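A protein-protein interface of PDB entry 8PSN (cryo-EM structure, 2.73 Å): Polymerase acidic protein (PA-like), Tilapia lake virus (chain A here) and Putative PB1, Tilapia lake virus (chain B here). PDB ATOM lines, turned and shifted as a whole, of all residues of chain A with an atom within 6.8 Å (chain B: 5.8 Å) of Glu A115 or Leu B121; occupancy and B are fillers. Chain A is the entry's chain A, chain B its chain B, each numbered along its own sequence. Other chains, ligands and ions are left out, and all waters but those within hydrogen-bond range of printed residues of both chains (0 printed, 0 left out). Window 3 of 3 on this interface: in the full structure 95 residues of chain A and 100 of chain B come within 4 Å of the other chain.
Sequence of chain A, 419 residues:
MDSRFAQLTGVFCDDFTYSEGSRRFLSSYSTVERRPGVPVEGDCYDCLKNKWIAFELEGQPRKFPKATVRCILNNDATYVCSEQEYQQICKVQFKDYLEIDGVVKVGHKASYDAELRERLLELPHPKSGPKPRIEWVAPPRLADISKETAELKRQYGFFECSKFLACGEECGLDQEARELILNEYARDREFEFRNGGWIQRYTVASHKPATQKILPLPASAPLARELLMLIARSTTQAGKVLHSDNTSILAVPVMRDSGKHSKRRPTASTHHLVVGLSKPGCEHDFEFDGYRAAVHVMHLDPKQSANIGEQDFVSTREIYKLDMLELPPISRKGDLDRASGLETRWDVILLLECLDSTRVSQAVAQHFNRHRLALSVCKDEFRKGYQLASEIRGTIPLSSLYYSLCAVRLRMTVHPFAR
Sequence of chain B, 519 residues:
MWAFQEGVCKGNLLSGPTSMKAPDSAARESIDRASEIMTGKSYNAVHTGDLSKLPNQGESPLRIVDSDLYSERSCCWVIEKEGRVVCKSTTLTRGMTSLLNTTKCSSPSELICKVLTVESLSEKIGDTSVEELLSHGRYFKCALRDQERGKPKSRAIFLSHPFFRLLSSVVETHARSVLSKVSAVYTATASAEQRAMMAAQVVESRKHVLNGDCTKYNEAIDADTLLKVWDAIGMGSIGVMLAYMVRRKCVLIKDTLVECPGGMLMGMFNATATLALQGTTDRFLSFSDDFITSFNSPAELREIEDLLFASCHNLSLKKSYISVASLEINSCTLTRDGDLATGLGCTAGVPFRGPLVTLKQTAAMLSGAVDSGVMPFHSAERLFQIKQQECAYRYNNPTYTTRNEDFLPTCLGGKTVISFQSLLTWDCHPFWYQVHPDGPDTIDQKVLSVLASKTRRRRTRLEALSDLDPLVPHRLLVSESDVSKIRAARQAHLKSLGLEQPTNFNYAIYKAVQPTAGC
The side-chain hydroxyl (OG) of Ser A111 is in hydrogen-bond range of the backbone carbonyl oxygen (O) of Val B118. The side-chain hydroxyl of Ser A111 sits at hydrogen-bond distance from the backbone carbonyl oxygen of Glu B119, 2.9 Å away. NH2 of Arg A119 is in salt-bridge range of OE1 of Glu B131 (2.9 Å).
OE2 of Glu A115 is in salt-bridge range of NH1 of Arg A119, at 3.6 Å. N of Glu B119 is in hydrogen-bond range of OE1 of Glu B123, 3.1 Å away. The side-chain hydroxyl of Ser B120 lies within hydrogen-bond range of the side-chain hydroxyl of Ser B122 (3.3 Å). The backbone NH (N) of Glu B123 lies within hydrogen-bond range of the side-chain hydroxyl (OG) of Ser B120 (3.4 Å). The backbone NH (N) of Glu B131 is in hydrogen-bond range of the backbone carbonyl oxygen (O) of Leu B121 (3.2 Å). OG of Ser B129 sits close to N of Glu B131, at 3.4 Å.
N of Ser B120 touches OG of Ser A111, 3.96 Å away. CG2 of Val B118 touches CE2 of Tyr A112, 3.7 Å away. CB of Tyr A112 touches CG of Leu B121, at 3.7 Å. Glu A115 touches Leu B121 (OE1 to CD1, 3.4 Å). CD1 of Leu B121 touches CD2 of Leu A116 (3.8 Å). Leu B134 touches Leu A116 (CD1 to CD1, 3.7 Å).
Of the printed residues of chain B, Ser A111 touches Val B118, Glu B119 and Ser B120. Of the printed residues of chain B, Tyr A112 touches Val B118 (3.7 Å) and Leu B121 (3.7 Å). Glu A115 touches one residue of chain B. Of the printed residues of chain A, Val B118 touches Ser A111 (2.9 Å) and Tyr A112 (3.7 Å). Of the printed residues of chain A, Glu B119 touches Ser A111. Of chain A, only Tyr A112, Glu A115 and Leu A116 come within 4 Å of Leu B121. Ser B129 touches none of the printed residues of chain A. Of the printed residues of chain A, Glu B131 touches Arg A119. The nearest printed residue of chain B that does not touch Glu A115 is Ser B120 (6.3 Å). The nearest residue of chain A that does not touch Leu B121 is Arg A119 (4.2 Å).
Of the 10 printed residues of chain A, 5 touch a printed residue of chain B. Printed residues of chain A that touch a printed residue of chain B: Ser A111, Tyr A112, Glu A115, Leu A116 and Arg A119. Hydrophobic or aromatic side chains of chain A that line the printed part of chain B: Tyr A112 and Leu A116.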
ATOM      1  N   SER A 111      22.258   7.077   8.966  1.00  0.00           N
ATOM      2  CA  SER A 111      23.058   8.275   9.199  1.00  0.00           C
ATOM      3  C   SER A 111      24.448   8.155   8.590  1.00  0.00           C
ATOM      4  O   SER A 111      25.061   9.172   8.247  1.00  0.00           O
ATOM      5  CB  SER A 111      23.164   8.548  10.699  1.00  0.00           C
ATOM      6  OG  SER A 111      23.450   7.358  11.413  1.00  0.00           O
ATOM      7  N   TYR A 112      24.957   6.935   8.442  1.00  0.00           N
ATOM      8  CA  TYR A 112      26.303   6.701   7.938  1.00  0.00           C
ATOM      9  C   TYR A 112      26.335   6.443   6.437  1.00  0.00           C
ATOM     10  O   TYR A 112      27.389   6.078   5.907  1.00  0.00           O
ATOM     11  CB  TYR A 112      26.947   5.523   8.677  1.00  0.00           C
ATOM     12  CG  TYR A 112      26.050   4.314   8.811  1.00  0.00           C
ATOM     13  CD1 TYR A 112      25.914   3.407   7.768  1.00  0.00           C
ATOM     14  CD2 TYR A 112      25.337   4.081   9.978  1.00  0.00           C
ATOM     15  CE1 TYR A 112      25.094   2.304   7.886  1.00  0.00           C
ATOM     16  CE2 TYR A 112      24.515   2.981  10.103  1.00  0.00           C
ATOM     17  CZ  TYR A 112      24.397   2.096   9.055  1.00  0.00           C
ATOM     18  OH  TYR A 112      23.579   0.998   9.179  1.00  0.00           O
ATOM     19  N   ASP A 113      25.210   6.622   5.743  1.00  0.00           N
ATOM     20  CA  ASP A 113      25.178   6.369   4.307  1.00  0.00           C
ATOM     21  C   ASP A 113      26.183   7.249   3.573  1.00  0.00           C
ATOM     22  O   ASP A 113      26.960   6.765   2.745  1.00  0.00           O
ATOM     23  CB  ASP A 113      23.763   6.603   3.772  1.00  0.00           C
ATOM     24  CG  ASP A 113      23.607   6.185   2.322  1.00  0.00           C
ATOM     25  OD1 ASP A 113      24.351   6.705   1.464  1.00  0.00           O
ATOM     26  OD2 ASP A 113      22.730   5.343   2.035  1.00  0.00           O
ATOM     27  N   ALA A 114      26.184   8.550   3.871  1.00  0.00           N
ATOM     28  CA  ALA A 114      27.081   9.465   3.173  1.00  0.00           C
ATOM     29  C   ALA A 114      28.540   9.148   3.473  1.00  0.00           C
ATOM     30  O   ALA A 114      29.390   9.196   2.577  1.00  0.00           O
ATOM     31  CB  ALA A 114      26.756  10.908   3.557  1.00  0.00           C
ATOM     32  N   GLU A 115      28.853   8.832   4.730  1.00  0.00           N
ATOM     33  CA  GLU A 115      30.232   8.528   5.097  1.00  0.00           C
ATOM     34  C   GLU A 115      30.730   7.283   4.372  1.00  0.00           C
ATOM     35  O   GLU A 115      31.848   7.260   3.840  1.00  0.00           O
ATOM     36  CB  GLU A 115      30.335   8.354   6.613  1.00  0.00           C
ATOM     37  CG  GLU A 115      31.540   7.559   7.077  1.00  0.00           C
ATOM     38  CD  GLU A 115      31.862   7.798   8.539  1.00  0.00           C
ATOM     39  OE1 GLU A 115      30.936   7.716   9.373  1.00  0.00           O
ATOM     40  OE2 GLU A 115      33.039   8.069   8.854  1.00  0.00           O
ATOM     41  N   LEU A 116      29.909   6.233   4.338  1.00  0.00           N
ATOM     42  CA  LEU A 116      30.310   5.009   3.652  1.00  0.00           C
ATOM     43  C   LEU A 116      30.412   5.231   2.150  1.00  0.00           C
ATOM     44  O   LEU A 116      31.286   4.657   1.492  1.00  0.00           O
ATOM     45  CB  LEU A 116      29.324   3.883   3.964  1.00  0.00           C
ATOM     46  CG  LEU A 116      29.377   3.254   5.361  1.00  0.00           C
ATOM     47  CD1 LEU A 116      28.672   1.909   5.352  1.00  0.00           C
ATOM     48  CD2 LEU A 116      30.802   3.094   5.869  1.00  0.00           C
ATOM     49  N   ARG A 117      29.531   6.060   1.587  1.00  0.00           N
ATOM     50  CA  ARG A 117      29.635   6.382   0.168  1.00  0.00           C
ATOM     51  C   ARG A 117      30.935   7.116  -0.131  1.00  0.00           C
ATOM     52  O   ARG A 117      31.592   6.843  -1.141  1.00  0.00           O
ATOM     53  CB  ARG A 117      28.430   7.211  -0.272  1.00  0.00           C
ATOM     54  CG  ARG A 117      27.149   6.405  -0.394  1.00  0.00           C
ATOM     55  CD  ARG A 117      26.225   6.971  -1.451  1.00  0.00           C
ATOM     56  NE  ARG A 117      24.905   6.352  -1.397  1.00  0.00           N
ATOM     57  CZ  ARG A 117      24.398   5.550  -2.326  1.00  0.00           C
ATOM     58  NH1 ARG A 117      25.074   5.231  -3.418  1.00  0.00           N
ATOM     59  NH2 ARG A 117      23.177   5.053  -2.154  1.00  0.00           N
ATOM     60  N   GLU A 118      31.324   8.051   0.737  1.00  0.00           N
ATOM     61  CA  GLU A 118      32.603   8.735   0.565  1.00  0.00           C
ATOM     62  C   GLU A 118      33.762   7.747   0.638  1.00  0.00           C
ATOM     63  O   GLU A 118      34.684   7.786  -0.189  1.00  0.00           O
ATOM     64  CB  GLU A 118      32.761   9.823   1.627  1.00  0.00           C
ATOM     65  CG  GLU A 118      32.461  11.227   1.134  1.00  0.00           C
ATOM     66  CD  GLU A 118      32.940  12.295   2.099  1.00  0.00           C
ATOM     67  OE1 GLU A 118      32.784  12.105   3.324  1.00  0.00           O
ATOM     68  OE2 GLU A 118      33.471  13.325   1.633  1.00  0.00           O
ATOM     69  N   ARG A 119      33.727   6.845   1.622  1.00  0.00           N
ATOM     70  CA  ARG A 119      34.788   5.852   1.747  1.00  0.00           C
ATOM     71  C   ARG A 119      34.881   4.992   0.495  1.00  0.00           C
ATOM     72  O   ARG A 119      35.980   4.714   0.001  1.00  0.00           O
ATOM     73  CB  ARG A 119      34.546   4.973   2.974  1.00  0.00           C
ATOM     74  CG  ARG A 119      35.047   5.566   4.279  1.00  0.00           C
ATOM     75  CD  ARG A 119      34.072   5.335   5.422  1.00  0.00           C
ATOM     76  NE  ARG A 119      34.338   4.078   6.113  1.00  0.00           N
ATOM     77  CZ  ARG A 119      34.669   3.963   7.394  1.00  0.00           C
ATOM     78  NH1 ARG A 119      34.791   5.019   8.181  1.00  0.00           N
ATOM     79  NH2 ARG A 119      34.885   2.751   7.898  1.00  0.00           N
ATOM     80  N   LEU A 120      33.735   4.559  -0.031  1.00  0.00           N
ATOM     81  CA  LEU A 120      33.732   3.743  -1.239  1.00  0.00           C
ATOM     82  C   LEU A 120      34.257   4.531  -2.430  1.00  0.00           C
ATOM     83  O   LEU A 120      34.958   3.983  -3.289  1.00  0.00           O
ATOM     84  CB  LEU A 120      32.317   3.227  -1.509  1.00  0.00           C
ATOM     85  CG  LEU A 120      32.129   2.294  -2.704  1.00  0.00           C
ATOM     86  CD1 LEU A 120      32.914   1.006  -2.518  1.00  0.00           C
ATOM     87  CD2 LEU A 120      30.657   1.995  -2.902  1.00  0.00           C
ATOM     88  N   VAL B 118      21.207   3.162  13.936  1.00  0.00           N
ATOM     89  CA  VAL B 118      22.246   3.598  14.864  1.00  0.00           C
ATOM     90  C   VAL B 118      22.751   4.957  14.403  1.00  0.00           C
ATOM     91  O   VAL B 118      23.001   5.163  13.210  1.00  0.00           O
ATOM     92  CB  VAL B 118      23.403   2.586  14.954  1.00  0.00           C
ATOM     93  CG1 VAL B 118      23.067   1.482  15.944  1.00  0.00           C
ATOM     94  CG2 VAL B 118      23.718   2.008  13.591  1.00  0.00           C
ATOM     95  N   GLU B 119      22.900   5.884  15.352  1.00  0.00           N
ATOM     96  CA  GLU B 119      23.262   7.256  15.015  1.00  0.00           C
ATOM     97  C   GLU B 119      24.656   7.371  14.409  1.00  0.00           C
ATOM     98  O   GLU B 119      24.935   8.363  13.729  1.00  0.00           O
ATOM     99  CB  GLU B 119      23.173   8.138  16.261  1.00  0.00           C
ATOM    100  CG  GLU B 119      21.771   8.269  16.829  1.00  0.00           C
ATOM    101  CD  GLU B 119      20.851   9.079  15.935  1.00  0.00           C
ATOM    102  OE1 GLU B 119      21.353   9.725  14.991  1.00  0.00           O
ATOM    103  OE2 GLU B 119      19.626   9.069  16.177  1.00  0.00           O
ATOM    104  N   SER B 120      25.534   6.396  14.637  1.00  0.00           N
ATOM    105  CA  SER B 120      26.893   6.475  14.121  1.00  0.00           C
ATOM    106  C   SER B 120      27.460   5.072  13.961  1.00  0.00           C
ATOM    107  O   SER B 120      26.942   4.101  14.517  1.00  0.00           O
ATOM    108  CB  SER B 120      27.795   7.308  15.040  1.00  0.00           C
ATOM    109  OG  SER B 120      27.970   6.673  16.294  1.00  0.00           O
ATOM    110  N   LEU B 121      28.543   4.982  13.185  1.00  0.00           N
ATOM    111  CA  LEU B 121      29.208   3.699  12.984  1.00  0.00           C
ATOM    112  C   LEU B 121      29.841   3.185  14.270  1.00  0.00           C
ATOM    113  O   LEU B 121      29.961   1.968  14.455  1.00  0.00           O
ATOM    114  CB  LEU B 121      30.275   3.828  11.896  1.00  0.00           C
ATOM    115  CG  LEU B 121      29.777   3.884  10.451  1.00  0.00           C
ATOM    116  CD1 LEU B 121      30.901   4.304   9.521  1.00  0.00           C
ATOM    117  CD2 LEU B 121      29.202   2.547  10.021  1.00  0.00           C
ATOM    118  N   SER B 122      30.249   4.084  15.165  1.00  0.00           N
ATOM    119  CA  SER B 122      30.922   3.688  16.394  1.00  0.00           C
ATOM    120  C   SER B 122      29.961   3.259  17.495  1.00  0.00           C
ATOM    121  O   SER B 122      30.410   2.672  18.485  1.00  0.00           O
ATOM    122  CB  SER B 122      31.793   4.838  16.904  1.00  0.00           C
ATOM    123  OG  SER B 122      31.205   6.092  16.607  1.00  0.00           O
ATOM    124  N   GLU B 123      28.666   3.528  17.353  1.00  0.00           N
ATOM    125  CA  GLU B 123      27.711   3.121  18.374  1.00  0.00           C
ATOM    126  C   GLU B 123      27.723   1.607  18.532  1.00  0.00           C
ATOM    127  O   GLU B 123      27.789   0.862  17.550  1.00  0.00           O
ATOM    128  CB  GLU B 123      26.307   3.605  18.011  1.00  0.00           C
ATOM    129  CG  GLU B 123      25.205   2.988  18.858  1.00  0.00           C
ATOM    130  CD  GLU B 123      23.884   3.716  18.718  1.00  0.00           C
ATOM    131  OE1 GLU B 123      23.849   4.766  18.042  1.00  0.00           O
ATOM    132  OE2 GLU B 123      22.878   3.236  19.281  1.00  0.00           O
ATOM    133  N   SER B 129      29.876  -3.241  16.883  1.00  0.00           N
ATOM    134  CA  SER B 129      29.373  -2.018  16.277  1.00  0.00           C
ATOM    135  C   SER B 129      29.271  -2.229  14.775  1.00  0.00           C
ATOM    136  O   SER B 129      29.779  -3.210  14.227  1.00  0.00           O
ATOM    137  CB  SER B 129      30.275  -0.821  16.597  1.00  0.00           C
ATOM    138  OG  SER B 129      31.474  -0.869  15.842  1.00  0.00           O
ATOM    139  N   VAL B 130      28.603  -1.292  14.100  1.00  0.00           N
ATOM    140  CA  VAL B 130      28.455  -1.395  12.651  1.00  0.00           C
ATOM    141  C   VAL B 130      29.818  -1.324  11.976  1.00  0.00           C
ATOM    142  O   VAL B 130      30.056  -1.983  10.959  1.00  0.00           O
ATOM    143  CB  VAL B 130      27.504  -0.304  12.127  1.00  0.00           C
ATOM    144  CG1 VAL B 130      27.450  -0.328  10.605  1.00  0.00           C
ATOM    145  CG2 VAL B 130      26.117  -0.491  12.709  1.00  0.00           C
ATOM    146  N   GLU B 131      30.729  -0.518  12.521  1.00  0.00           N
ATOM    147  CA  GLU B 131      32.083  -0.461  11.979  1.00  0.00           C
ATOM    148  C   GLU B 131      32.762  -1.823  12.076  1.00  0.00           C
ATOM    149  O   GLU B 131      33.333  -2.321  11.097  1.00  0.00           O
ATOM    150  CB  GLU B 131      32.888   0.609  12.723  1.00  0.00           C
ATOM    151  CG  GLU B 131      34.383   0.629  12.425  1.00  0.00           C
ATOM    152  CD  GLU B 131      34.696   1.173  11.047  1.00  0.00           C
ATOM    153  OE1 GLU B 131      33.796   1.767  10.419  1.00  0.00           O
ATOM    154  OE2 GLU B 131      35.847   1.009  10.592  1.00  0.00           O
ATOM    155  N   GLU B 132      32.699  -2.447  13.253  1.00  0.00           N
ATOM    156  CA  GLU B 132      33.299  -3.766  13.425  1.00  0.00           C
ATOM    157  C   GLU B 132      32.593  -4.809  12.570  1.00  0.00           C
ATOM    158  O   GLU B 132      33.240  -5.702  12.011  1.00  0.00           O
ATOM    159  CB  GLU B 132      33.268  -4.166  14.898  1.00  0.00           C
ATOM    160  CG  GLU B 132      34.125  -5.377  15.228  1.00  0.00           C
ATOM    161  CD  GLU B 132      34.578  -5.396  16.675  1.00  0.00           C
ATOM    162  OE1 GLU B 132      33.931  -4.730  17.511  1.00  0.00           O
ATOM    163  OE2 GLU B 132      35.582  -6.076  16.977  1.00  0.00           O
ATOM    164  N   LEU B 134      31.107  -4.326   9.662  1.00  0.00           N
ATOM    165  CA  LEU B 134      31.546  -4.137   8.286  1.00  0.00           C
ATOM    166  C   LEU B 134      32.973  -4.629   8.094  1.00  0.00           C
ATOM    167  O   LEU B 134      33.301  -5.213   7.055  1.00  0.00           O
ATOM    168  CB  LEU B 134      31.432  -2.664   7.897  1.00  0.00           C
ATOM    169  CG  LEU B 134      30.009  -2.125   7.750  1.00  0.00           C
ATOM    170  CD1 LEU B 134      30.016  -0.607   7.733  1.00  0.00           C
ATOM    171  CD2 LEU B 134      29.351  -2.674   6.495  1.00  0.00           C
